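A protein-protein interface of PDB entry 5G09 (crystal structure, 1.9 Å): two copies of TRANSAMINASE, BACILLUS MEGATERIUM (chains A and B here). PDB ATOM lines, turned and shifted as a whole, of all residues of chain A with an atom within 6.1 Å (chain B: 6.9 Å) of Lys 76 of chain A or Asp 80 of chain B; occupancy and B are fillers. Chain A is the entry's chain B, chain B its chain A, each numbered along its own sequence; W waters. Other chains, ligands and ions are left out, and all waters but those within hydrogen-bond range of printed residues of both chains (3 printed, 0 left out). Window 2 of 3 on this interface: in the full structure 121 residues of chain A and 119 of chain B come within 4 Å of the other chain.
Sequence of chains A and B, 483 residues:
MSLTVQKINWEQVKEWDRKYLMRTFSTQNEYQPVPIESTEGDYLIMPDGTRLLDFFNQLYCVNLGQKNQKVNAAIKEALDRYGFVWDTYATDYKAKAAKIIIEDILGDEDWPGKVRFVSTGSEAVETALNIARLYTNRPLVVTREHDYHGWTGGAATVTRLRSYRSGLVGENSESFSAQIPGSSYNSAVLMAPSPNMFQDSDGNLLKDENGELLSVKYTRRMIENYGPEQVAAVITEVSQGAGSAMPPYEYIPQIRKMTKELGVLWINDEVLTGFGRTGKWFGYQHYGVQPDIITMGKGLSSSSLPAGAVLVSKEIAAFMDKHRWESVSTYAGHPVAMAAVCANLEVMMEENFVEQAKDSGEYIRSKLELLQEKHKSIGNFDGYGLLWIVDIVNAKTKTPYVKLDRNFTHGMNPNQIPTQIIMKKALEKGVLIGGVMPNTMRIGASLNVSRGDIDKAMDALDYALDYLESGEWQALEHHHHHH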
ATOM      1  N   SER A  38      -6.965   8.767   8.755  1.00  0.00           N
ATOM      2  CA  SER A  38      -7.994   8.875   9.799  1.00  0.00           C
ATOM      3  C   SER A  38      -7.301   9.141  11.112  1.00  0.00           C
ATOM      4  O   SER A  38      -6.068   9.080  11.188  1.00  0.00           O
ATOM      5  CB  SER A  38      -8.883   7.601   9.867  1.00  0.00           C
ATOM      6  OG  SER A  38      -8.084   6.435  10.015  1.00  0.00           O
ATOM      7  N   LYS A  67     -11.762  12.463  16.898  1.00  0.00           N
ATOM      8  CA  LYS A  67     -12.908  11.690  16.376  1.00  0.00           C
ATOM      9  C   LYS A  67     -13.717  11.067  17.537  1.00  0.00           C
ATOM     10  O   LYS A  67     -13.931   9.853  17.591  1.00  0.00           O
ATOM     11  CB  LYS A  67     -12.454  10.624  15.347  1.00  0.00           C
ATOM     12  CG  LYS A  67     -13.596  10.006  14.501  1.00  0.00           C
ATOM     13  CD  LYS A  67     -13.094   8.917  13.548  1.00  0.00           C
ATOM     14  CE  LYS A  67     -12.725   7.614  14.264  1.00  0.00           C
ATOM     15  NZ  LYS A  67     -11.632   6.847  13.564  1.00  0.00           N
ATOM     16  N   VAL A  71     -19.417  13.549  19.965  1.00  0.00           N
ATOM     17  CA  VAL A  71     -19.408  14.787  19.187  1.00  0.00           C
ATOM     18  C   VAL A  71     -19.789  14.510  17.739  1.00  0.00           C
ATOM     19  O   VAL A  71     -20.636  15.208  17.187  1.00  0.00           O
ATOM     20  CB  VAL A  71     -18.046  15.527  19.233  1.00  0.00           C
ATOM     21  CG1 VAL A  71     -18.099  16.767  18.329  1.00  0.00           C
ATOM     22  CG2 VAL A  71     -17.688  15.914  20.668  1.00  0.00           C
ATOM     23  N   ASN A  72     -19.176  13.509  17.113  1.00  0.00           N
ATOM     24  CA  ASN A  72     -19.479  13.258  15.693  1.00  0.00           C
ATOM     25  C   ASN A  72     -20.957  12.866  15.469  1.00  0.00           C
ATOM     26  O   ASN A  72     -21.576  13.305  14.510  1.00  0.00           O
ATOM     27  CB  ASN A  72     -18.467  12.290  15.069  1.00  0.00           C
ATOM     28  CG  ASN A  72     -17.096  12.945  14.800  1.00  0.00           C
ATOM     29  OD1 ASN A  72     -16.786  14.018  15.330  1.00  0.00           O
ATOM     30  ND2 ASN A  72     -16.273  12.295  13.960  1.00  0.00           N
ATOM     31  N   ALA A  73     -21.539  12.104  16.397  1.00  0.00           N
ATOM     32  CA  ALA A  73     -22.970  11.798  16.311  1.00  0.00           C
ATOM     33  C   ALA A  73     -23.808  13.046  16.450  1.00  0.00           C
ATOM     34  O   ALA A  73     -24.806  13.198  15.748  1.00  0.00           O
ATOM     35  CB  ALA A  73     -23.398  10.769  17.344  1.00  0.00           C
ATOM     36  N   ALA A  74     -23.412  13.958  17.346  1.00  0.00           N
ATOM     37  CA  ALA A  74     -24.193  15.174  17.503  1.00  0.00           C
ATOM     38  C   ALA A  74     -24.079  16.043  16.232  1.00  0.00           C
ATOM     39  O   ALA A  74     -25.031  16.706  15.873  1.00  0.00           O
ATOM     40  CB  ALA A  74     -23.733  15.962  18.732  1.00  0.00           C
ATOM     41  N   ILE A  75     -22.925  16.032  15.558  1.00  0.00           N
ATOM     42  CA  ILE A  75     -22.791  16.800  14.320  1.00  0.00           C
ATOM     43  C   ILE A  75     -23.724  16.203  13.243  1.00  0.00           C
ATOM     44  O   ILE A  75     -24.427  16.944  12.542  1.00  0.00           O
ATOM     45  CB  ILE A  75     -21.325  16.852  13.819  1.00  0.00           C
ATOM     46  CG1 ILE A  75     -20.446  17.618  14.840  1.00  0.00           C
ATOM     47  CG2 ILE A  75     -21.267  17.527  12.437  1.00  0.00           C
ATOM     48  CD1 ILE A  75     -18.954  17.575  14.589  1.00  0.00           C
ATOM     49  N   LYS A  76     -23.738  14.858  13.144  1.00  0.00           N
ATOM     50  CA  LYS A  76     -24.582  14.143  12.164  1.00  0.00           C
ATOM     51  C   LYS A  76     -26.050  14.470  12.397  1.00  0.00           C
ATOM     52  O   LYS A  76     -26.813  14.639  11.445  1.00  0.00           O
ATOM     53  CB  LYS A  76     -24.366  12.622  12.230  1.00  0.00           C
ATOM     54  CG  LYS A  76     -23.036  12.164  11.633  1.00  0.00           C
ATOM     55  CD  LYS A  76     -22.824  10.659  11.802  1.00  0.00           C
ATOM     56  CE  LYS A  76     -21.533  10.202  11.150  1.00  0.00           C
ATOM     57  NZ  LYS A  76     -21.192   8.780  11.461  1.00  0.00           N
ATOM     58  N   GLU A  77     -26.424  14.563  13.671  1.00  0.00           N
ATOM     59  CA  GLU A  77     -27.775  14.918  14.062  1.00  0.00           C
ATOM     60  C   GLU A  77     -28.172  16.308  13.601  1.00  0.00           C
ATOM     61  O   GLU A  77     -29.287  16.516  13.110  1.00  0.00           O
ATOM     62  CB  GLU A  77     -27.932  14.831  15.568  1.00  0.00           C
ATOM     63  CG  GLU A  77     -28.202  13.428  16.057  1.00  0.00           C
ATOM     64  CD  GLU A  77     -29.305  13.400  17.098  1.00  0.00           C
ATOM     65  OE1 GLU A  77     -29.792  14.490  17.499  1.00  0.00           O
ATOM     66  OE2 GLU A  77     -29.691  12.281  17.507  1.00  0.00           O
ATOM     67  N   ALA A  78     -27.277  17.276  13.791  1.00  0.00           N
ATOM     68  CA  ALA A  78     -27.565  18.659  13.354  1.00  0.00           C
ATOM     69  C   ALA A  78     -27.774  18.728  11.844  1.00  0.00           C
ATOM     70  O   ALA A  78     -28.539  19.562  11.336  1.00  0.00           O
ATOM     71  CB  ALA A  78     -26.415  19.579  13.763  1.00  0.00           C
ATOM     72  N   LEU A  79     -27.079  17.851  11.130  1.00  0.00           N
ATOM     73  CA  LEU A  79     -27.188  17.798   9.672  1.00  0.00           C
ATOM     74  C   LEU A  79     -28.562  17.297   9.168  1.00  0.00           C
ATOM     75  O   LEU A  79     -28.858  17.412   7.977  1.00  0.00           O
ATOM     76  CB  LEU A  79     -26.032  16.993   9.069  1.00  0.00           C
ATOM     77  CG  LEU A  79     -24.612  17.624   9.148  1.00  0.00           C
ATOM     78  CD1 LEU A  79     -23.574  16.559   8.813  1.00  0.00           C
ATOM     79  CD2 LEU A  79     -24.386  18.845   8.257  1.00  0.00           C
ATOM     80  N   ASP A  80     -29.400  16.773  10.070  1.00  0.00           N
ATOM     81  CA  ASP A  80     -30.796  16.479   9.711  1.00  0.00           C
ATOM     82  C   ASP A  80     -31.637  17.734   9.599  1.00  0.00           C
ATOM     83  O   ASP A  80     -32.696  17.711   8.979  1.00  0.00           O
ATOM     84  CB  ASP A  80     -31.439  15.554  10.737  1.00  0.00           C
ATOM     85  CG  ASP A  80     -30.871  14.135  10.694  1.00  0.00           C
ATOM     86  OD1 ASP A  80     -30.185  13.746   9.717  1.00  0.00           O
ATOM     87  OD2 ASP A  80     -31.108  13.416  11.685  1.00  0.00           O
ATOM     88  N   ASN B  72     -24.470  16.612   2.728  1.00  0.00           N
ATOM     89  CA  ASN B  72     -24.577  16.152   4.103  1.00  0.00           C
ATOM     90  C   ASN B  72     -24.123  14.718   4.307  1.00  0.00           C
ATOM     91  O   ASN B  72     -23.481  14.410   5.312  1.00  0.00           O
ATOM     92  CB  ASN B  72     -25.988  16.436   4.639  1.00  0.00           C
ATOM     93  CG  ASN B  72     -26.163  17.892   5.021  1.00  0.00           C
ATOM     94  OD1 ASN B  72     -25.416  18.756   4.570  1.00  0.00           O
ATOM     95  ND2 ASN B  72     -27.132  18.172   5.856  1.00  0.00           N
ATOM     96  N   ILE B  75     -20.331  14.709   4.313  1.00  0.00           N
ATOM     97  CA  ILE B  75     -19.841  15.171   5.644  1.00  0.00           C
ATOM     98  C   ILE B  75     -19.912  14.043   6.671  1.00  0.00           C
ATOM     99  O   ILE B  75     -18.957  13.798   7.392  1.00  0.00           O
ATOM    100  CB  ILE B  75     -20.579  16.425   6.166  1.00  0.00           C
ATOM    101  CG1 ILE B  75     -20.353  17.606   5.202  1.00  0.00           C
ATOM    102  CG2 ILE B  75     -20.097  16.777   7.587  1.00  0.00           C
ATOM    103  CD1 ILE B  75     -21.308  18.768   5.402  1.00  0.00           C
ATOM    104  N   LYS B  76     -21.048  13.352   6.740  1.00  0.00           N
ATOM    105  CA  LYS B  76     -21.152  12.174   7.615  1.00  0.00           C
ATOM    106  C   LYS B  76     -20.076  11.106   7.329  1.00  0.00           C
ATOM    107  O   LYS B  76     -19.489  10.543   8.258  1.00  0.00           O
ATOM    108  CB  LYS B  76     -22.585  11.594   7.556  1.00  0.00           C
ATOM    109  CG  LYS B  76     -23.657  12.564   8.066  1.00  0.00           C
ATOM    110  CD  LYS B  76     -25.058  11.916   8.146  1.00  0.00           C
ATOM    111  CE  LYS B  76     -26.153  12.943   8.419  1.00  0.00           C
ATOM    112  NZ  LYS B  76     -27.489  12.332   8.711  1.00  0.00           N
ATOM    113  N   GLU B  77     -19.764  10.852   6.058  1.00  0.00           N
ATOM    114  CA  GLU B  77     -18.707   9.905   5.745  1.00  0.00           C
ATOM    115  C   GLU B  77     -17.366  10.372   6.226  1.00  0.00           C
ATOM    116  O   GLU B  77     -16.588   9.559   6.738  1.00  0.00           O
ATOM    117  CB  GLU B  77     -18.604   9.621   4.256  1.00  0.00           C
ATOM    118  CG  GLU B  77     -19.715   8.740   3.749  1.00  0.00           C
ATOM    119  CD  GLU B  77     -19.609   8.486   2.254  1.00  0.00           C
ATOM    120  OE1 GLU B  77     -18.565   8.821   1.632  1.00  0.00           O
ATOM    121  OE2 GLU B  77     -20.586   7.943   1.716  1.00  0.00           O
ATOM    122  N   ALA B  78     -17.086  11.670   6.059  1.00  0.00           N
ATOM    123  CA  ALA B  78     -15.827  12.236   6.541  1.00  0.00           C
ATOM    124  C   ALA B  78     -15.701  12.044   8.044  1.00  0.00           C
ATOM    125  O   ALA B  78     -14.619  11.771   8.552  1.00  0.00           O
ATOM    126  CB  ALA B  78     -15.695  13.727   6.174  1.00  0.00           C
ATOM    127  N   LEU B  79     -16.821  12.182   8.742  1.00  0.00           N
ATOM    128  CA  LEU B  79     -16.868  12.066  10.195  1.00  0.00           C
ATOM    129  C   LEU B  79     -16.680  10.630  10.698  1.00  0.00           C
ATOM    130  O   LEU B  79     -16.529  10.409  11.897  1.00  0.00           O
ATOM    131  CB  LEU B  79     -18.164  12.668  10.737  1.00  0.00           C
ATOM    132  CG  LEU B  79     -18.256  14.191  10.593  1.00  0.00           C
ATOM    133  CD1 LEU B  79     -19.702  14.624  10.765  1.00  0.00           C
ATOM    134  CD2 LEU B  79     -17.340  14.890  11.609  1.00  0.00           C
ATOM    135  N   ASP B  80     -16.679   9.674   9.780  1.00  0.00           N
ATOM    136  CA  ASP B  80     -16.318   8.299  10.129  1.00  0.00           C
ATOM    137  C   ASP B  80     -14.805   8.133  10.122  1.00  0.00           C
ATOM    138  O   ASP B  80     -14.310   7.111  10.528  1.00  0.00           O
ATOM    139  CB  ASP B  80     -16.933   7.306   9.144  1.00  0.00           C
ATOM    140  CG  ASP B  80     -18.416   7.153   9.335  1.00  0.00           C
ATOM    141  OD1 ASP B  80     -18.923   7.469  10.427  1.00  0.00           O
ATOM    142  OD2 ASP B  80     -19.092   6.737   8.373  1.00  0.00           O
ATOM    143  N   ARG B  81     -14.082   9.132   9.631  1.00  0.00           N
ATOM    144  CA  ARG B  81     -12.628   9.045   9.506  1.00  0.00           C
ATOM    145  C   ARG B  81     -11.959  10.103  10.386  1.00  0.00           C
ATOM    146  O   ARG B  81     -10.911   9.854  10.988  1.00  0.00           O
ATOM    147  CB  ARG B  81     -12.201   9.196   8.057  1.00  0.00           C
ATOM    148  CG  ARG B  81     -12.400   7.939   7.207  1.00  0.00           C
ATOM    149  CD  ARG B  81     -12.176   8.200   5.728  1.00  0.00           C
ATOM    150  NE  ARG B  81     -10.841   8.746   5.443  1.00  0.00           N
ATOM    151  CZ  ARG B  81     -10.527   9.431   4.346  1.00  0.00           C
ATOM    152  NH1 ARG B  81     -11.457   9.686   3.421  1.00  0.00           N
ATOM    153  NH2 ARG B  81      -9.286   9.881   4.172  1.00  0.00           N
ATOM    154  N   TYR B  82     -12.572  11.285  10.474  1.00  0.00           N
ATOM    155  CA  TYR B  82     -11.905  12.414  11.132  1.00  0.00           C
ATOM    156  C   TYR B  82     -12.850  12.977  12.182  1.00  0.00           C
ATOM    157  O   TYR B  82     -14.062  12.758  12.093  1.00  0.00           O
ATOM    158  CB  TYR B  82     -11.560  13.487  10.079  1.00  0.00           C
ATOM    159  CG  TYR B  82     -10.564  13.070   9.023  1.00  0.00           C
ATOM    160  CD1 TYR B  82      -9.185  12.996   9.301  1.00  0.00           C
ATOM    161  CD2 TYR B  82     -10.985  12.789   7.720  1.00  0.00           C
ATOM    162  CE1 TYR B  82      -8.279  12.624   8.315  1.00  0.00           C
ATOM    163  CE2 TYR B  82     -10.092  12.437   6.732  1.00  0.00           C
ATOM    164  CZ  TYR B  82      -8.755  12.349   7.009  1.00  0.00           C
ATOM    165  OH  TYR B  82      -7.901  11.997   5.971  1.00  0.00           O
ATOM    166  N   GLY B  83     -12.341  13.666  13.201  1.00  0.00           N
ATOM    167  CA  GLY B  83     -10.926  13.931  13.385  1.00  0.00           C
ATOM    168  C   GLY B  83     -10.546  15.328  12.936  1.00  0.00           C
ATOM    169  O   GLY B  83     -11.377  16.103  12.375  1.00  0.00           O
HETATM  170  O   HOH W   1     -11.970  15.284  16.185  1.00  0.00           O
HETATM  171  O   HOH W   2     -14.471  15.079  14.950  1.00  0.00           O
HETATM  172  O   HOH W   3     -11.837   5.857  10.736  1.00  0.00           O
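Water W2 bridges the side-chain amide oxygen (OD1) of Asn 72 of chain A (2.6 Å) and the backbone NH (N) of Gly 83 of chain B (3.1 Å).
Water W3 bridges O of Asp 80 of chain B (2.8 Å) and NZ of Lys 67 of chain A (3.0 Å).
Water W1 bridges the backbone NH of Lys 67 of chain A (2.9 Å) and the backbone NH of Gly 83 of chain B (3.4 Å).
Asn 72 of chain A touches Leu 79 of chain B, and with the chains exchanged Leu 79 of chain A touches Asn 72 of chain B.
Ile 75 of chain A touches Leu 79 of chain B, and with the chains exchanged Leu 79 of chain A touches Ile 75 of chain B.
Lys 76 of chain A touches its own counterpart, Lys 76 of chain B.
Lys 76 of chain A touches Asp 80 of chain B, and with the chains exchanged Asp 80 of chain A touches Lys 76 of chain B.
Positions printed for both chains: 72, 75, 76, 77, 78, 79 and 80.
Of the 14 pairs that touch across the chains among the printed residues, 7 have their exchanged pair printed and touching as well.
The side-chain carboxylate (OD1) of Asp 80 of chain B is in salt-bridge range of the side-chain amino group (NZ) of Lys 76 of chain A, 2.8 Å away.
O of Leu 79 of chain B is in hydrogen-bond range of ND2 of Asn 72 of chain A, 2.8 Å away.
ND2 of Asn 72 of chain A lies within hydrogen-bond range of O of Tyr 82 of chain B (2.9 Å).
The side-chain carboxylate (OD1) of Asp 80 of chain A is in salt-bridge range of the side-chain amino group (NZ) of Lys 76 of chain B (3.2 Å).
The side-chain amide nitrogen (ND2) of Asn 72 of chain B is in hydrogen-bond range of the backbone carbonyl oxygen (O) of Leu 79 of chain A, 2.8 Å away.
Of chain B, only Lys 76 and Asp 80 come within 4 Å of Lys 76 of chain A.
Of chain A, only Lys 67 and Lys 76 come within 4 Å of Asp 80 of chain B.
Of the printed residues of chain B, Asp 80 of chain A touches Lys 76 (3.2 Å).
Of the printed residues of chain A, Arg 81 of chain B touches Ser 38 and Lys 67.
Of the printed residues of chain A, Leu 79 of chain B touches Lys 67, Asn 72 and Ile 75.
Of the printed residues of chain A, Tyr 82 of chain B touches Lys 67 and Asn 72.
Ala 74 of chain A touches none of the printed residues of chain B.
Of the 10 printed residues of chain B, 8 touch a printed residue of chain A.
Hydrophobic or aromatic side chains of chain B that line the printed part of chain A: Ile 75 and Leu 79.
Along chain A the printed residues that touch a printed residue of chain B span positions 38 to 80.
Among the printed residues, Asp or Glu carboxylates within 4 Å of a Lys or Arg side-chain nitrogen of the other chain: Lys 76 of chain A with Asp 80 of chain B (2.8 Å) and Asp 80 of chain A with Lys 76 of chain B (3.2 Å).
The guanidinium group (NH2) of Arg 81 of chain B is in hydrogen-bond range of the side-chain hydroxyl (OH) of Tyr 82 of chain B, at 3.1 Å.
Among the printed residues, pairs that only touch across the chains: Ser 38 of chain A with Arg 81 of chain B, Lys 67 of chain A with Leu 79 of chain B, Lys 67 of chain A with Asp 80 of chain B, Lys 67 of chain A with Arg 81 of chain B, Lys 67 of chain A with Tyr 82 of chain B, Lys 67 of chain A with Gly 83 of chain B, Ile 75 of chain A with Leu 79 of chain B, Lys 76 of chain A with Lys 76 of chain B and Leu 79 of chain A with Ile 75 of chain B.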
